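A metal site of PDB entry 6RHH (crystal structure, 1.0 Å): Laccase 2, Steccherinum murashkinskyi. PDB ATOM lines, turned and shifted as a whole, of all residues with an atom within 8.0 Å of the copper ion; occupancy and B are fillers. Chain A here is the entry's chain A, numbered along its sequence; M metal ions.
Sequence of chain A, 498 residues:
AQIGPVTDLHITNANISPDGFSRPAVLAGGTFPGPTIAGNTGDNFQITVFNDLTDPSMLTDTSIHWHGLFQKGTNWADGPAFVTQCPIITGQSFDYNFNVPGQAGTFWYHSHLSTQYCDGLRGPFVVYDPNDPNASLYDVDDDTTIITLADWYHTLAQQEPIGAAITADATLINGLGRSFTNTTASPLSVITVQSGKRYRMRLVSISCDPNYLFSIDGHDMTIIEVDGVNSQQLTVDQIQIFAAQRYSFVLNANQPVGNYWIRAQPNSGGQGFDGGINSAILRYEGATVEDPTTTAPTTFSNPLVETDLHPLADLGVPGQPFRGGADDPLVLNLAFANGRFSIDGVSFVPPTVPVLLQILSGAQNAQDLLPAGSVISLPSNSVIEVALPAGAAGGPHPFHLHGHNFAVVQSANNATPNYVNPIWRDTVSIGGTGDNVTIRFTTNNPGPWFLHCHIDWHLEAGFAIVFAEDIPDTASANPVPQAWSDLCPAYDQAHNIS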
ATOM      1  N   CYS A 208       4.805 -16.796 -14.434  1.00  0.00           N
ATOM      2  CA  CYS A 208       3.567 -16.136 -14.831  1.00  0.00           C
ATOM      3  C   CYS A 208       2.972 -15.210 -13.760  1.00  0.00           C
ATOM      4  O   CYS A 208       2.044 -14.457 -14.059  1.00  0.00           O
ATOM      5  CB  CYS A 208       2.462 -17.108 -15.232  1.00  0.00           C
ATOM      6  SG  CYS A 208       2.514 -17.413 -17.032  1.00  0.00           S
ATOM      7  N   ASP A 209       3.452 -15.305 -12.519  1.00  0.00           N
ATOM      8  CA  ASP A 209       2.811 -14.543 -11.440  1.00  0.00           C
ATOM      9  C   ASP A 209       3.746 -14.357 -10.251  1.00  0.00           C
ATOM     10  O   ASP A 209       4.211 -13.244 -10.027  1.00  0.00           O
ATOM     11  CB  ASP A 209       1.441 -15.131 -11.081  1.00  0.00           C
ATOM     12  CG  ASP A 209       0.767 -14.521  -9.911  1.00  0.00           C
ATOM     13  OD1 ASP A 209       1.292 -13.696  -9.208  1.00  0.00           O
ATOM     14  OD2 ASP A 209      -0.346 -15.053  -9.585  1.00  0.00           O
ATOM     15  N   PHE A 341      -7.984  -4.578 -14.980  1.00  0.00           N
ATOM     16  CA  PHE A 341      -7.010  -3.537 -14.790  1.00  0.00           C
ATOM     17  C   PHE A 341      -7.184  -2.425 -15.812  1.00  0.00           C
ATOM     18  O   PHE A 341      -7.685  -2.635 -16.912  1.00  0.00           O
ATOM     19  CB  PHE A 341      -5.607  -4.100 -14.898  1.00  0.00           C
ATOM     20  CG  PHE A 341      -5.222  -4.975 -13.743  1.00  0.00           C
ATOM     21  CD1 PHE A 341      -5.410  -6.334 -13.769  1.00  0.00           C
ATOM     22  CD2 PHE A 341      -4.670  -4.410 -12.601  1.00  0.00           C
ATOM     23  CE1 PHE A 341      -5.055  -7.144 -12.685  1.00  0.00           C
ATOM     24  CE2 PHE A 341      -4.318  -5.204 -11.524  1.00  0.00           C
ATOM     25  CZ  PHE A 341      -4.519  -6.563 -11.544  1.00  0.00           C
ATOM     26  N   ALA A 392      -2.872  -0.555  -6.920  1.00  0.00           N
ATOM     27  CA  ALA A 392      -3.816  -1.473  -7.552  1.00  0.00           C
ATOM     28  C   ALA A 392      -3.703  -2.862  -6.933  1.00  0.00           C
ATOM     29  O   ALA A 392      -2.575  -3.342  -6.705  1.00  0.00           O
ATOM     30  CB  ALA A 392      -3.540  -1.571  -9.051  1.00  0.00           C
ATOM     31  N   ALA A 393      -4.843  -3.517  -6.714  1.00  0.00           N
ATOM     32  CA  ALA A 393      -4.884  -4.867  -6.164  1.00  0.00           C
ATOM     33  C   ALA A 393      -3.993  -5.812  -6.951  1.00  0.00           C
ATOM     34  O   ALA A 393      -3.737  -5.660  -8.141  1.00  0.00           O
ATOM     35  CB  ALA A 393      -6.325  -5.352  -6.161  1.00  0.00           C
ATOM     36  N   GLY A 394      -3.595  -6.867  -6.246  1.00  0.00           N
ATOM     37  CA  GLY A 394      -2.826  -7.930  -6.831  1.00  0.00           C
ATOM     38  C   GLY A 394      -1.328  -7.683  -6.888  1.00  0.00           C
ATOM     39  O   GLY A 394      -0.615  -8.410  -7.546  1.00  0.00           O
ATOM     40  N   GLY A 395      -0.870  -6.658  -6.185  1.00  0.00           N
ATOM     41  CA  GLY A 395       0.555  -6.311  -6.202  1.00  0.00           C
ATOM     42  C   GLY A 395       1.384  -7.297  -5.386  1.00  0.00           C
ATOM     43  O   GLY A 395       0.859  -8.163  -4.678  1.00  0.00           O
ATOM     44  N   PRO A 396       2.711  -7.123  -5.421  1.00  0.00           N
ATOM     45  CA  PRO A 396       3.439  -6.064  -6.135  1.00  0.00           C
ATOM     46  C   PRO A 396       3.578  -6.416  -7.631  1.00  0.00           C
ATOM     47  O   PRO A 396       3.920  -7.526  -8.026  1.00  0.00           O
ATOM     48  CB  PRO A 396       4.804  -6.065  -5.448  1.00  0.00           C
ATOM     49  CG  PRO A 396       4.942  -7.457  -4.947  1.00  0.00           C
ATOM     50  CD  PRO A 396       3.595  -7.920  -4.576  1.00  0.00           C
ATOM     51  N   HIS A 397       3.275  -5.408  -8.450  1.00  0.00           N
ATOM     52  CA  HIS A 397       3.220  -5.596  -9.905  1.00  0.00           C
ATOM     53  C   HIS A 397       4.576  -5.346 -10.541  1.00  0.00           C
ATOM     54  O   HIS A 397       5.116  -4.243 -10.425  1.00  0.00           O
ATOM     55  CB  HIS A 397       2.215  -4.642 -10.524  1.00  0.00           C
ATOM     56  CG  HIS A 397       0.839  -4.800  -9.991  1.00  0.00           C
ATOM     57  ND1 HIS A 397       0.011  -5.849 -10.373  1.00  0.00           N
ATOM     58  CD2 HIS A 397       0.140  -4.019  -9.130  1.00  0.00           C
ATOM     59  CE1 HIS A 397      -1.115  -5.686  -9.692  1.00  0.00           C
ATOM     60  NE2 HIS A 397      -1.066  -4.623  -8.957  1.00  0.00           N
ATOM     61  N   PRO A 398       5.129  -6.345 -11.285  1.00  0.00           N
ATOM     62  CA  PRO A 398       6.398  -6.142 -11.992  1.00  0.00           C
ATOM     63  C   PRO A 398       6.138  -5.604 -13.404  1.00  0.00           C
ATOM     64  O   PRO A 398       5.760  -6.346 -14.322  1.00  0.00           O
ATOM     65  CB  PRO A 398       7.004  -7.553 -12.004  1.00  0.00           C
ATOM     66  CG  PRO A 398       5.801  -8.474 -12.068  1.00  0.00           C
ATOM     67  CD  PRO A 398       4.700  -7.753 -11.325  1.00  0.00           C
ATOM     68  N   PHE A 399       6.343  -4.307 -13.581  1.00  0.00           N
ATOM     69  CA  PHE A 399       6.131  -3.668 -14.874  1.00  0.00           C
ATOM     70  C   PHE A 399       7.346  -3.837 -15.772  1.00  0.00           C
ATOM     71  O   PHE A 399       8.490  -3.699 -15.346  1.00  0.00           O
ATOM     72  CB  PHE A 399       5.744  -2.177 -14.740  1.00  0.00           C
ATOM     73  CG  PHE A 399       4.267  -1.988 -14.694  1.00  0.00           C
ATOM     74  CD1 PHE A 399       3.513  -2.395 -13.602  1.00  0.00           C
ATOM     75  CD2 PHE A 399       3.585  -1.491 -15.817  1.00  0.00           C
ATOM     76  CE1 PHE A 399       2.108  -2.312 -13.632  1.00  0.00           C
ATOM     77  CE2 PHE A 399       2.207  -1.419 -15.839  1.00  0.00           C
ATOM     78  CZ  PHE A 399       1.483  -1.822 -14.767  1.00  0.00           C
ATOM     79  N   ILE A 430       6.764  -2.351  -8.902  1.00  0.00           N
ATOM     80  CA  ILE A 430       6.296  -0.997  -8.543  1.00  0.00           C
ATOM     81  C   ILE A 430       5.923  -0.909  -7.070  1.00  0.00           C
ATOM     82  O   ILE A 430       5.540   0.174  -6.577  1.00  0.00           O
ATOM     83  CB  ILE A 430       5.197  -0.494  -9.474  1.00  0.00           C
ATOM     84  CG1 ILE A 430       3.883  -1.224  -9.295  1.00  0.00           C
ATOM     85  CG2 ILE A 430       5.685  -0.523 -10.917  1.00  0.00           C
ATOM     86  CD1 ILE A 430       2.716  -0.570 -10.035  1.00  0.00           C
ATOM     87  N   HIS A 452       3.648  -3.237 -19.732  1.00  0.00           N
ATOM     88  CA  HIS A 452       2.624  -3.986 -19.038  1.00  0.00           C
ATOM     89  C   HIS A 452       3.134  -4.617 -17.791  1.00  0.00           C
ATOM     90  O   HIS A 452       4.328  -4.835 -17.618  1.00  0.00           O
ATOM     91  CB  HIS A 452       2.034  -5.067 -19.999  1.00  0.00           C
ATOM     92  CG  HIS A 452       3.003  -6.109 -20.448  1.00  0.00           C
ATOM     93  ND1 HIS A 452       3.271  -7.247 -19.718  1.00  0.00           N
ATOM     94  CD2 HIS A 452       3.767  -6.197 -21.562  1.00  0.00           C
ATOM     95  CE1 HIS A 452       4.145  -7.979 -20.397  1.00  0.00           C
ATOM     96  NE2 HIS A 452       4.485  -7.374 -21.525  1.00  0.00           N
ATOM     97  N   CYS A 453       2.188  -4.979 -16.923  1.00  0.00           N
ATOM     98  CA  CYS A 453       2.520  -5.847 -15.803  1.00  0.00           C
ATOM     99  C   CYS A 453       2.861  -7.226 -16.324  1.00  0.00           C
ATOM    100  O   CYS A 453       2.149  -7.759 -17.202  1.00  0.00           O
ATOM    101  CB  CYS A 453       1.328  -5.934 -14.840  1.00  0.00           C
ATOM    102  SG  CYS A 453       1.792  -6.987 -13.413  1.00  0.00           S
ATOM    103  N   HIS A 454       3.925  -7.841 -15.816  1.00  0.00           N
ATOM    104  CA  HIS A 454       4.374  -9.153 -16.273  1.00  0.00           C
ATOM    105  C   HIS A 454       3.766 -10.308 -15.493  1.00  0.00           C
ATOM    106  O   HIS A 454       4.119 -11.453 -15.756  1.00  0.00           O
ATOM    107  CB  HIS A 454       5.910  -9.244 -16.313  1.00  0.00           C
ATOM    108  CG  HIS A 454       6.404 -10.033 -17.495  1.00  0.00           C
ATOM    109  ND1 HIS A 454       6.147 -11.360 -17.692  1.00  0.00           N
ATOM    110  CD2 HIS A 454       7.147  -9.686 -18.556  1.00  0.00           C
ATOM    111  CE1 HIS A 454       6.726 -11.759 -18.825  1.00  0.00           C
ATOM    112  NE2 HIS A 454       7.364 -10.752 -19.391  1.00  0.00           N
ATOM    113  N   ILE A 455       2.831 -10.044 -14.579  1.00  0.00           N
ATOM    114  CA  ILE A 455       1.953 -11.104 -14.065  1.00  0.00           C
ATOM    115  C   ILE A 455       0.979 -11.357 -15.215  1.00  0.00           C
ATOM    116  O   ILE A 455       0.168 -10.492 -15.567  1.00  0.00           O
ATOM    117  CB  ILE A 455       1.295 -10.699 -12.744  1.00  0.00           C
ATOM    118  CG1 ILE A 455       2.347 -10.524 -11.658  1.00  0.00           C
ATOM    119  CG2 ILE A 455       0.228 -11.716 -12.361  1.00  0.00           C
ATOM    120  CD1 ILE A 455       1.864  -9.813 -10.395  1.00  0.00           C
ATOM    121  N   ASP A 456       1.092 -12.533 -15.824  1.00  0.00           N
ATOM    122  CA  ASP A 456       0.396 -12.742 -17.085  1.00  0.00           C
ATOM    123  C   ASP A 456      -1.099 -12.672 -16.953  1.00  0.00           C
ATOM    124  O   ASP A 456      -1.816 -12.254 -17.853  1.00  0.00           O
ATOM    125  CB  ASP A 456       0.898 -14.058 -17.718  1.00  0.00           C
ATOM    126  CG  ASP A 456       0.928 -14.043 -19.253  1.00  0.00           C
ATOM    127  OD1 ASP A 456       1.218 -12.956 -19.787  1.00  0.00           O
ATOM    128  OD2 ASP A 456       0.716 -15.110 -19.832  1.00  0.00           O
ATOM    129  N   TRP A 457      -1.608 -13.100 -15.777  1.00  0.00           N
ATOM    130  CA  TRP A 457      -3.029 -13.022 -15.513  1.00  0.00           C
ATOM    131  C   TRP A 457      -3.503 -11.562 -15.502  1.00  0.00           C
ATOM    132  O   TRP A 457      -4.652 -11.275 -15.837  1.00  0.00           O
ATOM    133  CB  TRP A 457      -3.375 -13.723 -14.167  1.00  0.00           C
ATOM    134  CG  TRP A 457      -2.702 -15.075 -14.032  1.00  0.00           C
ATOM    135  CD1 TRP A 457      -1.720 -15.387 -13.129  1.00  0.00           C
ATOM    136  CD2 TRP A 457      -2.930 -16.230 -14.816  1.00  0.00           C
ATOM    137  NE1 TRP A 457      -1.317 -16.691 -13.324  1.00  0.00           N
ATOM    138  CE2 TRP A 457      -2.046 -17.240 -14.345  1.00  0.00           C
ATOM    139  CE3 TRP A 457      -3.821 -16.560 -15.828  1.00  0.00           C
ATOM    140  CZ2 TRP A 457      -2.010 -18.507 -14.896  1.00  0.00           C
ATOM    141  CZ3 TRP A 457      -3.786 -17.783 -16.352  1.00  0.00           C
ATOM    142  CH2 TRP A 457      -2.882 -18.773 -15.887  1.00  0.00           C
ATOM    143  N   HIS A 458      -2.647 -10.640 -15.086  1.00  0.00           N
ATOM    144  CA  HIS A 458      -2.979  -9.228 -15.050  1.00  0.00           C
ATOM    145  C   HIS A 458      -2.898  -8.585 -16.448  1.00  0.00           C
ATOM    146  O   HIS A 458      -3.738  -7.761 -16.795  1.00  0.00           O
ATOM    147  CB  HIS A 458      -2.044  -8.486 -14.081  1.00  0.00           C
ATOM    148  CG  HIS A 458      -2.151  -8.941 -12.680  1.00  0.00           C
ATOM    149  ND1 HIS A 458      -1.321  -8.403 -11.710  1.00  0.00           N
ATOM    150  CD2 HIS A 458      -2.971  -9.837 -12.111  1.00  0.00           C
ATOM    151  CE1 HIS A 458      -1.665  -9.012 -10.573  1.00  0.00           C
ATOM    152  NE2 HIS A 458      -2.653  -9.864 -10.767  1.00  0.00           N
ATOM    153  N   LEU A 459      -1.900  -8.991 -17.247  1.00  0.00           N
ATOM    154  CA  LEU A 459      -1.868  -8.578 -18.641  1.00  0.00           C
ATOM    155  C   LEU A 459      -3.152  -8.995 -19.333  1.00  0.00           C
ATOM    156  O   LEU A 459      -3.778  -8.191 -20.066  1.00  0.00           O
ATOM    157  CB  LEU A 459      -0.639  -9.163 -19.330  1.00  0.00           C
ATOM    158  CG  LEU A 459      -0.566  -8.997 -20.846  1.00  0.00           C
ATOM    159  CD1 LEU A 459      -0.639  -7.554 -21.273  1.00  0.00           C
ATOM    160  CD2 LEU A 459       0.660  -9.674 -21.396  1.00  0.00           C
ATOM    161  N   PHE A 463      -3.869  -4.998 -18.029  1.00  0.00           N
ATOM    162  CA  PHE A 463      -2.909  -4.091 -17.359  1.00  0.00           C
ATOM    163  C   PHE A 463      -1.735  -3.743 -18.288  1.00  0.00           C
ATOM    164  O   PHE A 463      -0.613  -4.206 -18.092  1.00  0.00           O
ATOM    165  CB  PHE A 463      -2.453  -4.664 -16.043  1.00  0.00           C
ATOM    166  CG  PHE A 463      -2.129  -3.709 -14.929  1.00  0.00           C
ATOM    167  CD1 PHE A 463      -2.481  -2.365 -14.952  1.00  0.00           C
ATOM    168  CD2 PHE A 463      -1.528  -4.189 -13.778  1.00  0.00           C
ATOM    169  CE1 PHE A 463      -2.273  -1.537 -13.846  1.00  0.00           C
ATOM    170  CE2 PHE A 463      -1.299  -3.383 -12.660  1.00  0.00           C
ATOM    171  CZ  PHE A 463      -1.688  -2.083 -12.694  1.00  0.00           C
HETATM  172 CU    CU M   1       0.181  -7.098 -11.966  1.00  0.00          CU
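O of His 458 is in hydrogen-bond range of N of Phe 463, 3.0 Å away.
A ring nitrogen (NE2) of His 397 lies within hydrogen-bond range of the backbone carbonyl oxygen (O) of Ala 393 (3.0 Å).
The backbone NH (N) of Gly 395 sits at hydrogen-bond distance from a ring nitrogen (NE2) of His 397, at 3.4 Å.
The backbone carbonyl oxygen of Ala 392 lies within hydrogen-bond range of a ring nitrogen (NE2) of His 397, 3.0 Å away.
The backbone carbonyl oxygen (O) of His 397 lies within hydrogen-bond range of the backbone NH (N) of Ile 430.
SG of Cys 453 sits close to N of Ile 455, 3.4 Å away.
O of Phe 463 sits at hydrogen-bond distance from N of Cys 453, at 3.1 Å.
A ring nitrogen (ND1) of His 458 binds the copper ion (2.0 Å).
The copper ion is bound by ND1 of His 397, at 2.0 Å.
The side-chain sulfur (SG) of Cys 453 binds the copper ion (2.2 Å).
The copper ion has three donor atoms within binding distance.
Merely in contact with the copper ion: Ile 455 and Phe 463.
Within 4 Å of the copper ion: His 397, Cys 453, Ile 455, His 458 and Phe 463.
The nearest printed residue that does not touch the copper ion is Pro 398 (4.6 Å).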
